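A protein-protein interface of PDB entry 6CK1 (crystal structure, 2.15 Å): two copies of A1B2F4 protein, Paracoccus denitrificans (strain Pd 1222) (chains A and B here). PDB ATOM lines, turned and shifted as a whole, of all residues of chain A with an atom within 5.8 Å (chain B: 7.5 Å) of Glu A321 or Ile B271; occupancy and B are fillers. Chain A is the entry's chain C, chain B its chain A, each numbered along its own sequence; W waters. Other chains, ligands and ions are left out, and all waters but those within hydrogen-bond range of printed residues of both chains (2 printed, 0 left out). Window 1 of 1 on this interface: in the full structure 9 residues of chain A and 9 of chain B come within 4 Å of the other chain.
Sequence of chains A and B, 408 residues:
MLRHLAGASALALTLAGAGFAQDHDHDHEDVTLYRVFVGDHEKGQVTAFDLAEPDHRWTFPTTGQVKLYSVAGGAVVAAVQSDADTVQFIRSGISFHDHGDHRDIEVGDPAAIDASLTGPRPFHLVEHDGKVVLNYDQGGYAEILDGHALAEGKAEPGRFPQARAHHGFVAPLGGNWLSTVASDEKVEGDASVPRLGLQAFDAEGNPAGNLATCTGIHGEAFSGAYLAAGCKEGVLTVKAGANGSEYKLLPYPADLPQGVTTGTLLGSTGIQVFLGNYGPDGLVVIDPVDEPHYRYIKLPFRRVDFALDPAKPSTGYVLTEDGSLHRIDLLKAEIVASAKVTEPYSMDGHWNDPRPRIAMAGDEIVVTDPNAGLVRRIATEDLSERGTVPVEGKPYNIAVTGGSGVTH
Of the printed residues of chain B, Pro A300 touches Ile B271 and Gln B272. Glu A321 touches just these residues of chain B: Ile B271 and Leu B331. Of the printed residues of chain B, Ser A346 touches Ser B314 and Leu B331. Gly B270 touches none of the printed residues of chain A. Of the printed residues of chain A, Gln B272 touches Pro A300. Of the printed residues of chain A, Leu B331 touches Phe A301 (3.9 Å), Glu A321 (3.5 Å), Pro A344 (3.5 Å) and Ser A346 (3.4 Å). The nearest residue of chain A that does not touch Ile B271 is Arg A302 (4.2 Å). The nearest printed residue of chain B that does not touch Asp A348 is Thr B315 (4.5 Å).
The backbone NH (N) of Ile B271 lies within hydrogen-bond range of the side-chain hydroxyl (OG) of Ser B268, 3.1 Å away. OG1 of Thr B315 lies within hydrogen-bond range of O of Lys B312. N of Leu B330 sits at hydrogen-bond distance from O of Ser B314, at 2.9 Å. NE of Arg A302 lies within salt-bridge range of OE2 of Glu A321, 2.8 Å away. NH2 of Arg A302 is in salt-bridge range of OD2 of Asp A348. The side-chain carboxylate (OE1) of Glu A321 sits at hydrogen-bond distance from the backbone NH (N) of Met A347.
The backbone carbonyl oxygen of Pro A300 is in hydrogen-bond range of the backbone NH of Gln B272, 2.9 Å away. The side-chain hydroxyl (OG) of Ser B314 sits at hydrogen-bond distance from the side-chain hydroxyl (OG) of Ser A346 (2.6 Å). The side-chain carboxylate (OD2) of Asp A348 is in hydrogen-bond range of the side-chain hydroxyl (OG) of Ser B314 (2.6 Å). The backbone carbonyl oxygen of Pro A344 is in hydrogen-bond range of the side-chain amino group of Lys B332, at 2.9 Å.
No position is printed for both chains.
Water W1 lies within hydrogen-bond range of the backbone carbonyl oxygen (O) of Gly B270 (2.9 Å) and the backbone carbonyl oxygen (O) of Pro A300 (3.5 Å). Water W2 lies within hydrogen-bond range of the backbone NH of Ser A346 and the side-chain amino group of Lys B332.
Of the 20 printed residues of chain B, 7 touch a printed residue of chain A. Of the 17 printed residues of chain A, 7 touch a printed residue of chain B. Printed residues of chain A that touch a printed residue of chain B: Pro A300, Phe A301, Arg A302, Glu A321, Pro A344, Ser A346 and Asp A348. Hydrophobic or aromatic side chains of chain A that line the printed part of chain B: Phe A301 and Pro A344. Among the printed residues, no Asp or Glu carboxylate lies within 4 Å of a Lys or Arg side-chain nitrogen of the other chain.
Among the printed residues, merely in contact across the chains: Pro A300 with Ile B271 (3.5 Å), Phe A301 with Ile B271 (3.9 Å), Phe A301 with Leu B331 (3.9 Å), Arg A302 with Pro B313 (3.4 Å), Arg A302 with Ser B314 (3.6 Å), Glu A321 with Ile B271 (3.3 Å), Glu A321 with Leu B331 (3.5 Å), Pro A344 with Leu B331 (3.5 Å), Ser A346 with Leu B331 (3.4 Å), Asp A348 with Lys B312 (3.4 Å) and Asp A348 with Pro B313 (3.6 Å).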
ATOM      1  N   PRO A 300      13.883  19.319 -27.700  1.00  0.00           N
ATOM      2  CA  PRO A 300      14.812  18.782 -28.721  1.00  0.00           C
ATOM      3  C   PRO A 300      16.222  18.481 -28.205  1.00  0.00           C
ATOM      4  O   PRO A 300      16.932  17.684 -28.825  1.00  0.00           O
ATOM      5  CB  PRO A 300      14.847  19.897 -29.775  1.00  0.00           C
ATOM      6  CG  PRO A 300      14.576  21.137 -28.977  1.00  0.00           C
ATOM      7  CD  PRO A 300      13.580  20.741 -27.929  1.00  0.00           C
ATOM      8  N   PHE A 301      16.645  19.109 -27.120  1.00  0.00           N
ATOM      9  CA  PHE A 301      17.881  18.818 -26.425  1.00  0.00           C
ATOM     10  C   PHE A 301      17.553  18.732 -24.941  1.00  0.00           C
ATOM     11  O   PHE A 301      16.478  19.140 -24.510  1.00  0.00           O
ATOM     12  CB  PHE A 301      18.942  19.894 -26.686  1.00  0.00           C
ATOM     13  CG  PHE A 301      19.345  20.039 -28.131  1.00  0.00           C
ATOM     14  CD1 PHE A 301      20.398  19.269 -28.647  1.00  0.00           C
ATOM     15  CD2 PHE A 301      18.716  20.953 -28.971  1.00  0.00           C
ATOM     16  CE1 PHE A 301      20.796  19.395 -29.981  1.00  0.00           C
ATOM     17  CE2 PHE A 301      19.102  21.072 -30.327  1.00  0.00           C
ATOM     18  CZ  PHE A 301      20.146  20.297 -30.823  1.00  0.00           C
ATOM     19  N   ARG A 302      18.461  18.171 -24.156  1.00  0.00           N
ATOM     20  CA  ARG A 302      18.145  17.915 -22.762  1.00  0.00           C
ATOM     21  C   ARG A 302      18.178  19.209 -21.956  1.00  0.00           C
ATOM     22  O   ARG A 302      18.839  20.179 -22.336  1.00  0.00           O
ATOM     23  CB  ARG A 302      19.088  16.863 -22.177  1.00  0.00           C
ATOM     24  CG  ARG A 302      18.771  15.486 -22.762  1.00  0.00           C
ATOM     25  CD  ARG A 302      19.848  14.487 -22.424  1.00  0.00           C
ATOM     26  NE  ARG A 302      21.124  14.911 -22.985  1.00  0.00           N
ATOM     27  CZ  ARG A 302      22.259  14.250 -22.831  1.00  0.00           C
ATOM     28  NH1 ARG A 302      22.262  13.118 -22.129  1.00  0.00           N
ATOM     29  NH2 ARG A 302      23.386  14.725 -23.385  1.00  0.00           N
ATOM     30  N   ARG A 303      17.424  19.216 -20.847  1.00  0.00           N
ATOM     31  CA  ARG A 303      17.219  20.410 -20.033  1.00  0.00           C
ATOM     32  C   ARG A 303      18.424  20.672 -19.133  1.00  0.00           C
ATOM     33  O   ARG A 303      18.863  19.790 -18.407  1.00  0.00           O
ATOM     34  CB  ARG A 303      15.948  20.254 -19.170  1.00  0.00           C
ATOM     35  CG  ARG A 303      15.558  21.490 -18.300  1.00  0.00           C
ATOM     36  CD  ARG A 303      14.267  21.181 -17.447  1.00  0.00           C
ATOM     37  NE  ARG A 303      14.596  20.079 -16.572  1.00  0.00           N
ATOM     38  CZ  ARG A 303      15.066  20.258 -15.346  1.00  0.00           C
ATOM     39  NH1 ARG A 303      15.179  21.493 -14.871  1.00  0.00           N
ATOM     40  NH2 ARG A 303      15.401  19.216 -14.604  1.00  0.00           N
ATOM     41  N   VAL A 304      18.892  21.913 -19.109  1.00  0.00           N
ATOM     42  CA  VAL A 304      19.947  22.336 -18.196  1.00  0.00           C
ATOM     43  C   VAL A 304      19.372  22.970 -16.933  1.00  0.00           C
ATOM     44  O   VAL A 304      19.850  22.710 -15.825  1.00  0.00           O
ATOM     45  CB  VAL A 304      20.909  23.311 -18.908  1.00  0.00           C
ATOM     46  CG1 VAL A 304      21.940  23.835 -17.925  1.00  0.00           C
ATOM     47  CG2 VAL A 304      21.561  22.652 -20.145  1.00  0.00           C
ATOM     48  N   LEU A 319      16.211  26.288 -20.393  1.00  0.00           N
ATOM     49  CA  LEU A 319      17.483  26.309 -21.104  1.00  0.00           C
ATOM     50  C   LEU A 319      17.913  24.870 -21.377  1.00  0.00           C
ATOM     51  O   LEU A 319      17.906  24.028 -20.469  1.00  0.00           O
ATOM     52  CB  LEU A 319      18.556  27.069 -20.313  1.00  0.00           C
ATOM     53  CG  LEU A 319      19.952  27.176 -20.959  1.00  0.00           C
ATOM     54  CD1 LEU A 319      19.959  28.128 -22.142  1.00  0.00           C
ATOM     55  CD2 LEU A 319      20.983  27.644 -19.926  1.00  0.00           C
ATOM     56  N   THR A 320      18.238  24.581 -22.633  1.00  0.00           N
ATOM     57  CA  THR A 320      18.649  23.236 -23.025  1.00  0.00           C
ATOM     58  C   THR A 320      20.121  23.241 -23.447  1.00  0.00           C
ATOM     59  O   THR A 320      20.744  24.294 -23.646  1.00  0.00           O
ATOM     60  CB  THR A 320      17.730  22.680 -24.119  1.00  0.00           C
ATOM     61  OG1 THR A 320      17.646  23.590 -25.204  1.00  0.00           O
ATOM     62  CG2 THR A 320      16.326  22.516 -23.566  1.00  0.00           C
ATOM     63  N   GLU A 321      20.669  22.029 -23.561  1.00  0.00           N
ATOM     64  CA  GLU A 321      22.110  21.798 -23.630  1.00  0.00           C
ATOM     65  C   GLU A 321      22.755  22.320 -24.906  1.00  0.00           C
ATOM     66  O   GLU A 321      23.983  22.407 -24.946  1.00  0.00           O
ATOM     67  CB  GLU A 321      22.394  20.300 -23.452  1.00  0.00           C
ATOM     68  CG  GLU A 321      21.861  19.419 -24.589  1.00  0.00           C
ATOM     69  CD  GLU A 321      22.009  17.929 -24.292  1.00  0.00           C
ATOM     70  OE1 GLU A 321      23.082  17.500 -23.780  1.00  0.00           O
ATOM     71  OE2 GLU A 321      21.035  17.181 -24.549  1.00  0.00           O
ATOM     72  N   ASP A 322      21.976  22.648 -25.943  1.00  0.00           N
ATOM     73  CA  ASP A 322      22.499  23.335 -27.118  1.00  0.00           C
ATOM     74  C   ASP A 322      22.715  24.825 -26.882  1.00  0.00           C
ATOM     75  O   ASP A 322      23.159  25.514 -27.803  1.00  0.00           O
ATOM     76  CB  ASP A 322      21.558  23.167 -28.315  1.00  0.00           C
ATOM     77  CG  ASP A 322      20.209  23.852 -28.074  1.00  0.00           C
ATOM     78  OD1 ASP A 322      19.826  23.948 -26.885  1.00  0.00           O
ATOM     79  OD2 ASP A 322      19.540  24.284 -29.043  1.00  0.00           O
ATOM     80  N   GLY A 323      22.385  25.342 -25.702  1.00  0.00           N
ATOM     81  CA  GLY A 323      22.505  26.755 -25.411  1.00  0.00           C
ATOM     82  C   GLY A 323      21.279  27.597 -25.713  1.00  0.00           C
ATOM     83  O   GLY A 323      21.339  28.828 -25.572  1.00  0.00           O
ATOM     84  N   SER A 324      20.162  26.972 -26.077  1.00  0.00           N
ATOM     85  CA  SER A 324      18.933  27.684 -26.376  1.00  0.00           C
ATOM     86  C   SER A 324      18.081  27.860 -25.126  1.00  0.00           C
ATOM     87  O   SER A 324      17.858  26.910 -24.369  1.00  0.00           O
ATOM     88  CB  SER A 324      18.112  26.925 -27.418  1.00  0.00           C
ATOM     89  OG  SER A 324      18.845  26.741 -28.606  1.00  0.00           O
ATOM     90  N   GLU A 343      26.912  29.156 -25.230  1.00  0.00           N
ATOM     91  CA  GLU A 343      27.456  28.013 -25.914  1.00  0.00           C
ATOM     92  C   GLU A 343      26.842  26.734 -25.347  1.00  0.00           C
ATOM     93  O   GLU A 343      26.304  26.724 -24.235  1.00  0.00           O
ATOM     94  CB  GLU A 343      28.975  27.991 -25.764  1.00  0.00           C
ATOM     95  CG  GLU A 343      29.415  27.562 -24.364  1.00  0.00           C
ATOM     96  CD  GLU A 343      30.879  27.846 -24.066  1.00  0.00           C
ATOM     97  OE1 GLU A 343      31.417  28.844 -24.591  1.00  0.00           O
ATOM     98  OE2 GLU A 343      31.481  27.084 -23.277  1.00  0.00           O
ATOM     99  N   PRO A 344      26.938  25.632 -26.086  1.00  0.00           N
ATOM    100  CA  PRO A 344      26.391  24.364 -25.592  1.00  0.00           C
ATOM    101  C   PRO A 344      27.091  23.898 -24.326  1.00  0.00           C
ATOM    102  O   PRO A 344      28.281  24.142 -24.120  1.00  0.00           O
ATOM    103  CB  PRO A 344      26.639  23.389 -26.753  1.00  0.00           C
ATOM    104  CG  PRO A 344      26.757  24.272 -27.985  1.00  0.00           C
ATOM    105  CD  PRO A 344      27.398  25.550 -27.488  1.00  0.00           C
ATOM    106  N   TYR A 345      26.325  23.205 -23.475  1.00  0.00           N
ATOM    107  CA  TYR A 345      26.828  22.591 -22.243  1.00  0.00           C
ATOM    108  C   TYR A 345      26.185  21.207 -22.152  1.00  0.00           C
ATOM    109  O   TYR A 345      25.027  21.090 -21.733  1.00  0.00           O
ATOM    110  CB  TYR A 345      26.491  23.418 -21.009  1.00  0.00           C
ATOM    111  CG  TYR A 345      27.349  24.636 -20.769  1.00  0.00           C
ATOM    112  CD1 TYR A 345      27.045  25.851 -21.354  1.00  0.00           C
ATOM    113  CD2 TYR A 345      28.458  24.572 -19.932  1.00  0.00           C
ATOM    114  CE1 TYR A 345      27.841  26.984 -21.128  1.00  0.00           C
ATOM    115  CE2 TYR A 345      29.242  25.689 -19.695  1.00  0.00           C
ATOM    116  CZ  TYR A 345      28.930  26.889 -20.290  1.00  0.00           C
ATOM    117  OH  TYR A 345      29.710  27.996 -20.031  1.00  0.00           O
ATOM    118  N   SER A 346      26.914  20.175 -22.572  1.00  0.00           N
ATOM    119  CA  SER A 346      26.362  18.820 -22.624  1.00  0.00           C
ATOM    120  C   SER A 346      25.800  18.369 -21.268  1.00  0.00           C
ATOM    121  O   SER A 346      26.416  18.567 -20.210  1.00  0.00           O
ATOM    122  CB  SER A 346      27.465  17.840 -23.075  1.00  0.00           C
ATOM    123  OG  SER A 346      27.052  16.494 -22.922  1.00  0.00           O
ATOM    124  N   MET A 347      24.654  17.692 -21.296  1.00  0.00           N
ATOM    125  CA  MET A 347      24.108  17.134 -20.061  1.00  0.00           C
ATOM    126  C   MET A 347      24.677  15.759 -19.723  1.00  0.00           C
ATOM    127  O   MET A 347      24.335  15.208 -18.665  1.00  0.00           O
ATOM    128  CB  MET A 347      22.556  17.076 -20.131  1.00  0.00           C
ATOM    129  CG  MET A 347      21.915  18.453 -19.931  1.00  0.00           C
ATOM    130  SD  MET A 347      22.569  19.323 -18.452  1.00  0.00           S
ATOM    131  CE  MET A 347      21.930  18.271 -17.136  1.00  0.00           C
ATOM    132  N   ASP A 348      25.530  15.200 -20.580  1.00  0.00           N
ATOM    133  CA  ASP A 348      26.338  14.043 -20.220  1.00  0.00           C
ATOM    134  C   ASP A 348      27.428  14.461 -19.235  1.00  0.00           C
ATOM    135  O   ASP A 348      27.942  15.580 -19.283  1.00  0.00           O
ATOM    136  CB  ASP A 348      26.925  13.430 -21.483  1.00  0.00           C
ATOM    137  CG  ASP A 348      25.847  12.815 -22.348  1.00  0.00           C
ATOM    138  OD1 ASP A 348      25.003  12.075 -21.803  1.00  0.00           O
ATOM    139  OD2 ASP A 348      25.764  13.160 -23.538  1.00  0.00           O
ATOM    140  N   PHE B 222      16.213   8.579 -38.828  1.00  0.00           N
ATOM    141  CA  PHE B 222      15.199   9.283 -38.052  1.00  0.00           C
ATOM    142  C   PHE B 222      15.808   9.900 -36.798  1.00  0.00           C
ATOM    143  O   PHE B 222      16.652   9.279 -36.138  1.00  0.00           O
ATOM    144  CB  PHE B 222      14.083   8.327 -37.613  1.00  0.00           C
ATOM    145  CG  PHE B 222      13.268   7.764 -38.744  1.00  0.00           C
ATOM    146  CD1 PHE B 222      13.675   6.613 -39.397  1.00  0.00           C
ATOM    147  CD2 PHE B 222      12.071   8.349 -39.106  1.00  0.00           C
ATOM    148  CE1 PHE B 222      12.915   6.074 -40.423  1.00  0.00           C
ATOM    149  CE2 PHE B 222      11.300   7.814 -40.131  1.00  0.00           C
ATOM    150  CZ  PHE B 222      11.733   6.673 -40.790  1.00  0.00           C
ATOM    151  N   SER B 223      15.339  11.090 -36.431  1.00  0.00           N
ATOM    152  CA  SER B 223      15.664  11.688 -35.136  1.00  0.00           C
ATOM    153  C   SER B 223      14.566  12.656 -34.708  1.00  0.00           C
ATOM    154  O   SER B 223      14.172  13.526 -35.492  1.00  0.00           O
ATOM    155  CB  SER B 223      16.991  12.443 -35.164  1.00  0.00           C
ATOM    156  OG  SER B 223      17.305  12.911 -33.866  1.00  0.00           O
ATOM    157  N   GLY B 224      14.111  12.524 -33.460  1.00  0.00           N
ATOM    158  CA  GLY B 224      13.052  13.404 -32.988  1.00  0.00           C
ATOM    159  C   GLY B 224      11.852  13.260 -33.899  1.00  0.00           C
ATOM    160  O   GLY B 224      11.333  12.162 -34.116  1.00  0.00           O
ATOM    161  N   GLY B 267      20.791   9.219 -36.890  1.00  0.00           N
ATOM    162  CA  GLY B 267      19.920  10.097 -36.124  1.00  0.00           C
ATOM    163  C   GLY B 267      19.961   9.791 -34.634  1.00  0.00           C
ATOM    164  O   GLY B 267      19.881   8.627 -34.240  1.00  0.00           O
ATOM    165  N   SER B 268      20.114  10.796 -33.793  1.00  0.00           N
ATOM    166  CA  SER B 268      20.147  10.502 -32.366  1.00  0.00           C
ATOM    167  C   SER B 268      18.771  10.067 -31.876  1.00  0.00           C
ATOM    168  O   SER B 268      17.754  10.648 -32.259  1.00  0.00           O
ATOM    169  CB  SER B 268      20.604  11.721 -31.570  1.00  0.00           C
ATOM    170  OG  SER B 268      20.552  11.434 -30.179  1.00  0.00           O
ATOM    171  N   THR B 269      18.748   9.073 -30.986  1.00  0.00           N
ATOM    172  CA  THR B 269      17.527   8.670 -30.283  1.00  0.00           C
ATOM    173  C   THR B 269      17.312   9.455 -28.993  1.00  0.00           C
ATOM    174  O   THR B 269      16.282   9.280 -28.339  1.00  0.00           O
ATOM    175  CB  THR B 269      17.564   7.170 -29.928  1.00  0.00           C
ATOM    176  OG1 THR B 269      18.760   6.889 -29.185  1.00  0.00           O
ATOM    177  CG2 THR B 269      17.526   6.288 -31.167  1.00  0.00           C
ATOM    178  N   GLY B 270      18.284  10.263 -28.590  1.00  0.00           N
ATOM    179  CA  GLY B 270      18.278  11.007 -27.343  1.00  0.00           C
ATOM    180  C   GLY B 270      17.992  12.487 -27.513  1.00  0.00           C
ATOM    181  O   GLY B 270      17.270  13.094 -26.712  1.00  0.00           O
ATOM    182  N   ILE B 271      18.704  13.120 -28.434  1.00  0.00           N
ATOM    183  CA  ILE B 271      18.426  14.497 -28.823  1.00  0.00           C
ATOM    184  C   ILE B 271      18.042  14.522 -30.303  1.00  0.00           C
ATOM    185  O   ILE B 271      18.135  13.516 -31.013  1.00  0.00           O
ATOM    186  CB  ILE B 271      19.605  15.417 -28.517  1.00  0.00           C
ATOM    187  CG1 ILE B 271      20.816  14.937 -29.299  1.00  0.00           C
ATOM    188  CG2 ILE B 271      19.893  15.356 -26.992  1.00  0.00           C
ATOM    189  CD1 ILE B 271      22.071  15.729 -28.993  1.00  0.00           C
ATOM    190  N   GLN B 272      17.554  15.674 -30.756  1.00  0.00           N
ATOM    191  CA  GLN B 272      17.051  15.804 -32.124  1.00  0.00           C
ATOM    192  C   GLN B 272      18.161  16.349 -33.010  1.00  0.00           C
ATOM    193  O   GLN B 272      18.310  17.569 -33.180  1.00  0.00           O
ATOM    194  CB  GLN B 272      15.820  16.702 -32.168  1.00  0.00           C
ATOM    195  CG  GLN B 272      15.169  16.750 -33.549  1.00  0.00           C
ATOM    196  CD  GLN B 272      13.839  17.503 -33.544  1.00  0.00           C
ATOM    197  OE1 GLN B 272      12.771  16.890 -33.531  1.00  0.00           O
ATOM    198  NE2 GLN B 272      13.907  18.838 -33.562  1.00  0.00           N
ATOM    199  N   VAL B 273      18.963  15.441 -33.572  1.00  0.00           N
ATOM    200  CA  VAL B 273      20.120  15.838 -34.371  1.00  0.00           C
ATOM    201  C   VAL B 273      20.522  14.663 -35.255  1.00  0.00           C
ATOM    202  O   VAL B 273      20.302  13.496 -34.914  1.00  0.00           O
ATOM    203  CB  VAL B 273      21.290  16.305 -33.468  1.00  0.00           C
ATOM    204  CG1 VAL B 273      21.995  15.093 -32.843  1.00  0.00           C
ATOM    205  CG2 VAL B 273      22.269  17.136 -34.259  1.00  0.00           C
ATOM    206  N   PHE B 274      21.098  14.980 -36.397  1.00  0.00           N
ATOM    207  CA  PHE B 274      21.658  13.999 -37.304  1.00  0.00           C
ATOM    208  C   PHE B 274      23.153  14.216 -37.449  1.00  0.00           C
ATOM    209  O   PHE B 274      23.649  15.348 -37.424  1.00  0.00           O
ATOM    210  CB  PHE B 274      21.037  14.080 -38.702  1.00  0.00           C
ATOM    211  CG  PHE B 274      19.588  13.811 -38.729  1.00  0.00           C
ATOM    212  CD1 PHE B 274      19.125  12.506 -38.797  1.00  0.00           C
ATOM    213  CD2 PHE B 274      18.678  14.850 -38.688  1.00  0.00           C
ATOM    214  CE1 PHE B 274      17.767  12.237 -38.814  1.00  0.00           C
ATOM    215  CE2 PHE B 274      17.312  14.595 -38.711  1.00  0.00           C
ATOM    216  CZ  PHE B 274      16.854  13.291 -38.777  1.00  0.00           C
ATOM    217  N   LEU B 308      26.471   6.568 -33.202  1.00  0.00           N
ATOM    218  CA  LEU B 308      26.067   7.503 -32.163  1.00  0.00           C
ATOM    219  C   LEU B 308      25.906   6.737 -30.854  1.00  0.00           C
ATOM    220  O   LEU B 308      25.594   5.539 -30.858  1.00  0.00           O
ATOM    221  CB  LEU B 308      24.748   8.217 -32.532  1.00  0.00           C
ATOM    222  CG  LEU B 308      24.833   9.090 -33.799  1.00  0.00           C
ATOM    223  CD1 LEU B 308      23.546   9.870 -34.016  1.00  0.00           C
ATOM    224  CD2 LEU B 308      26.013  10.039 -33.732  1.00  0.00           C
ATOM    225  N   PRO B 310      23.799   6.097 -27.794  1.00  0.00           N
ATOM    226  CA  PRO B 310      22.513   6.381 -27.147  1.00  0.00           C
ATOM    227  C   PRO B 310      22.616   6.538 -25.648  1.00  0.00           C
ATOM    228  O   PRO B 310      21.763   7.220 -25.063  1.00  0.00           O
ATOM    229  CB  PRO B 310      21.633   5.177 -27.528  1.00  0.00           C
ATOM    230  CG  PRO B 310      22.587   4.079 -27.808  1.00  0.00           C
ATOM    231  CD  PRO B 310      23.813   4.766 -28.421  1.00  0.00           C
ATOM    232  N   LYS B 312      24.981   8.163 -24.195  1.00  0.00           N
ATOM    233  CA  LYS B 312      25.539   9.499 -24.019  1.00  0.00           C
ATOM    234  C   LYS B 312      25.187  10.314 -25.255  1.00  0.00           C
ATOM    235  O   LYS B 312      26.056  10.649 -26.072  1.00  0.00           O
ATOM    236  CB  LYS B 312      27.043   9.390 -23.766  1.00  0.00           C
ATOM    237  CG  LYS B 312      27.349   8.491 -22.554  1.00  0.00           C
ATOM    238  CD  LYS B 312      26.947   9.227 -21.257  1.00  0.00           C
ATOM    239  CE  LYS B 312      27.127   8.383 -20.000  1.00  0.00           C
ATOM    240  NZ  LYS B 312      28.547   8.064 -19.770  1.00  0.00           N
ATOM    241  N   PRO B 313      23.916  10.696 -25.398  1.00  0.00           N
ATOM    242  CA  PRO B 313      23.425  11.161 -26.719  1.00  0.00           C
ATOM    243  C   PRO B 313      24.052  12.454 -27.244  1.00  0.00           C
ATOM    244  O   PRO B 313      23.783  12.804 -28.400  1.00  0.00           O
ATOM    245  CB  PRO B 313      21.912  11.322 -26.499  1.00  0.00           C
ATOM    246  CG  PRO B 313      21.728  11.383 -24.989  1.00  0.00           C
ATOM    247  CD  PRO B 313      22.826  10.537 -24.411  1.00  0.00           C
ATOM    248  N   SER B 314      24.859  13.187 -26.464  1.00  0.00           N
ATOM    249  CA  SER B 314      25.516  14.326 -27.072  1.00  0.00           C
ATOM    250  C   SER B 314      26.839  13.921 -27.734  1.00  0.00           C
ATOM    251  O   SER B 314      27.551  14.784 -28.250  1.00  0.00           O
ATOM    252  CB  SER B 314      25.795  15.417 -26.036  1.00  0.00           C
ATOM    253  OG  SER B 314      26.776  15.011 -25.085  1.00  0.00           O
ATOM    254  N   THR B 315      27.122  12.623 -27.830  1.00  0.00           N
ATOM    255  CA  THR B 315      28.393  12.145 -28.347  1.00  0.00           C
ATOM    256  C   THR B 315      28.172  11.045 -29.376  1.00  0.00           C
ATOM    257  O   THR B 315      27.145  10.350 -29.382  1.00  0.00           O
ATOM    258  CB  THR B 315      29.341  11.581 -27.242  1.00  0.00           C
ATOM    259  OG1 THR B 315      28.785  10.381 -26.702  1.00  0.00           O
ATOM    260  CG2 THR B 315      29.596  12.581 -26.081  1.00  0.00           C
ATOM    261  N   LEU B 330      28.688  16.202 -30.501  1.00  0.00           N
ATOM    262  CA  LEU B 330      27.653  16.626 -31.436  1.00  0.00           C
ATOM    263  C   LEU B 330      27.152  18.044 -31.149  1.00  0.00           C
ATOM    264  O   LEU B 330      26.660  18.725 -32.061  1.00  0.00           O
ATOM    265  CB  LEU B 330      26.485  15.643 -31.374  1.00  0.00           C
ATOM    266  CG  LEU B 330      26.806  14.185 -31.722  1.00  0.00           C
ATOM    267  CD1 LEU B 330      25.606  13.254 -31.404  1.00  0.00           C
ATOM    268  CD2 LEU B 330      27.178  14.094 -33.205  1.00  0.00           C
ATOM    269  N   LEU B 331      27.216  18.484 -29.891  1.00  0.00           N
ATOM    270  CA  LEU B 331      26.687  19.803 -29.536  1.00  0.00           C
ATOM    271  C   LEU B 331      27.593  20.914 -30.046  1.00  0.00           C
ATOM    272  O   LEU B 331      27.118  21.915 -30.580  1.00  0.00           O
ATOM    273  CB  LEU B 331      26.527  19.907 -28.016  1.00  0.00           C
ATOM    274  CG  LEU B 331      25.547  18.896 -27.395  1.00  0.00           C
ATOM    275  CD1 LEU B 331      25.396  19.088 -25.855  1.00  0.00           C
ATOM    276  CD2 LEU B 331      24.224  19.046 -28.090  1.00  0.00           C
ATOM    277  N   LYS B 332      28.905  20.771 -29.850  1.00  0.00           N
ATOM    278  CA  LYS B 332      29.876  21.715 -30.388  1.00  0.00           C
ATOM    279  C   LYS B 332      30.361  21.348 -31.791  1.00  0.00           C
ATOM    280  O   LYS B 332      31.033  22.163 -32.431  1.00  0.00           O
ATOM    281  CB  LYS B 332      31.050  21.866 -29.427  1.00  0.00           C
ATOM    282  CG  LYS B 332      30.667  22.644 -28.175  1.00  0.00           C
ATOM    283  CD  LYS B 332      31.755  22.628 -27.119  1.00  0.00           C
ATOM    284  CE  LYS B 332      31.395  23.582 -25.970  1.00  0.00           C
ATOM    285  NZ  LYS B 332      30.894  22.920 -24.733  1.00  0.00           N
HETATM  286  O   HOH W   1      15.211  15.064 -27.349  1.00  0.00           O
HETATM  287  O   HOH W   2      29.780  20.622 -23.013  1.00  0.00           O
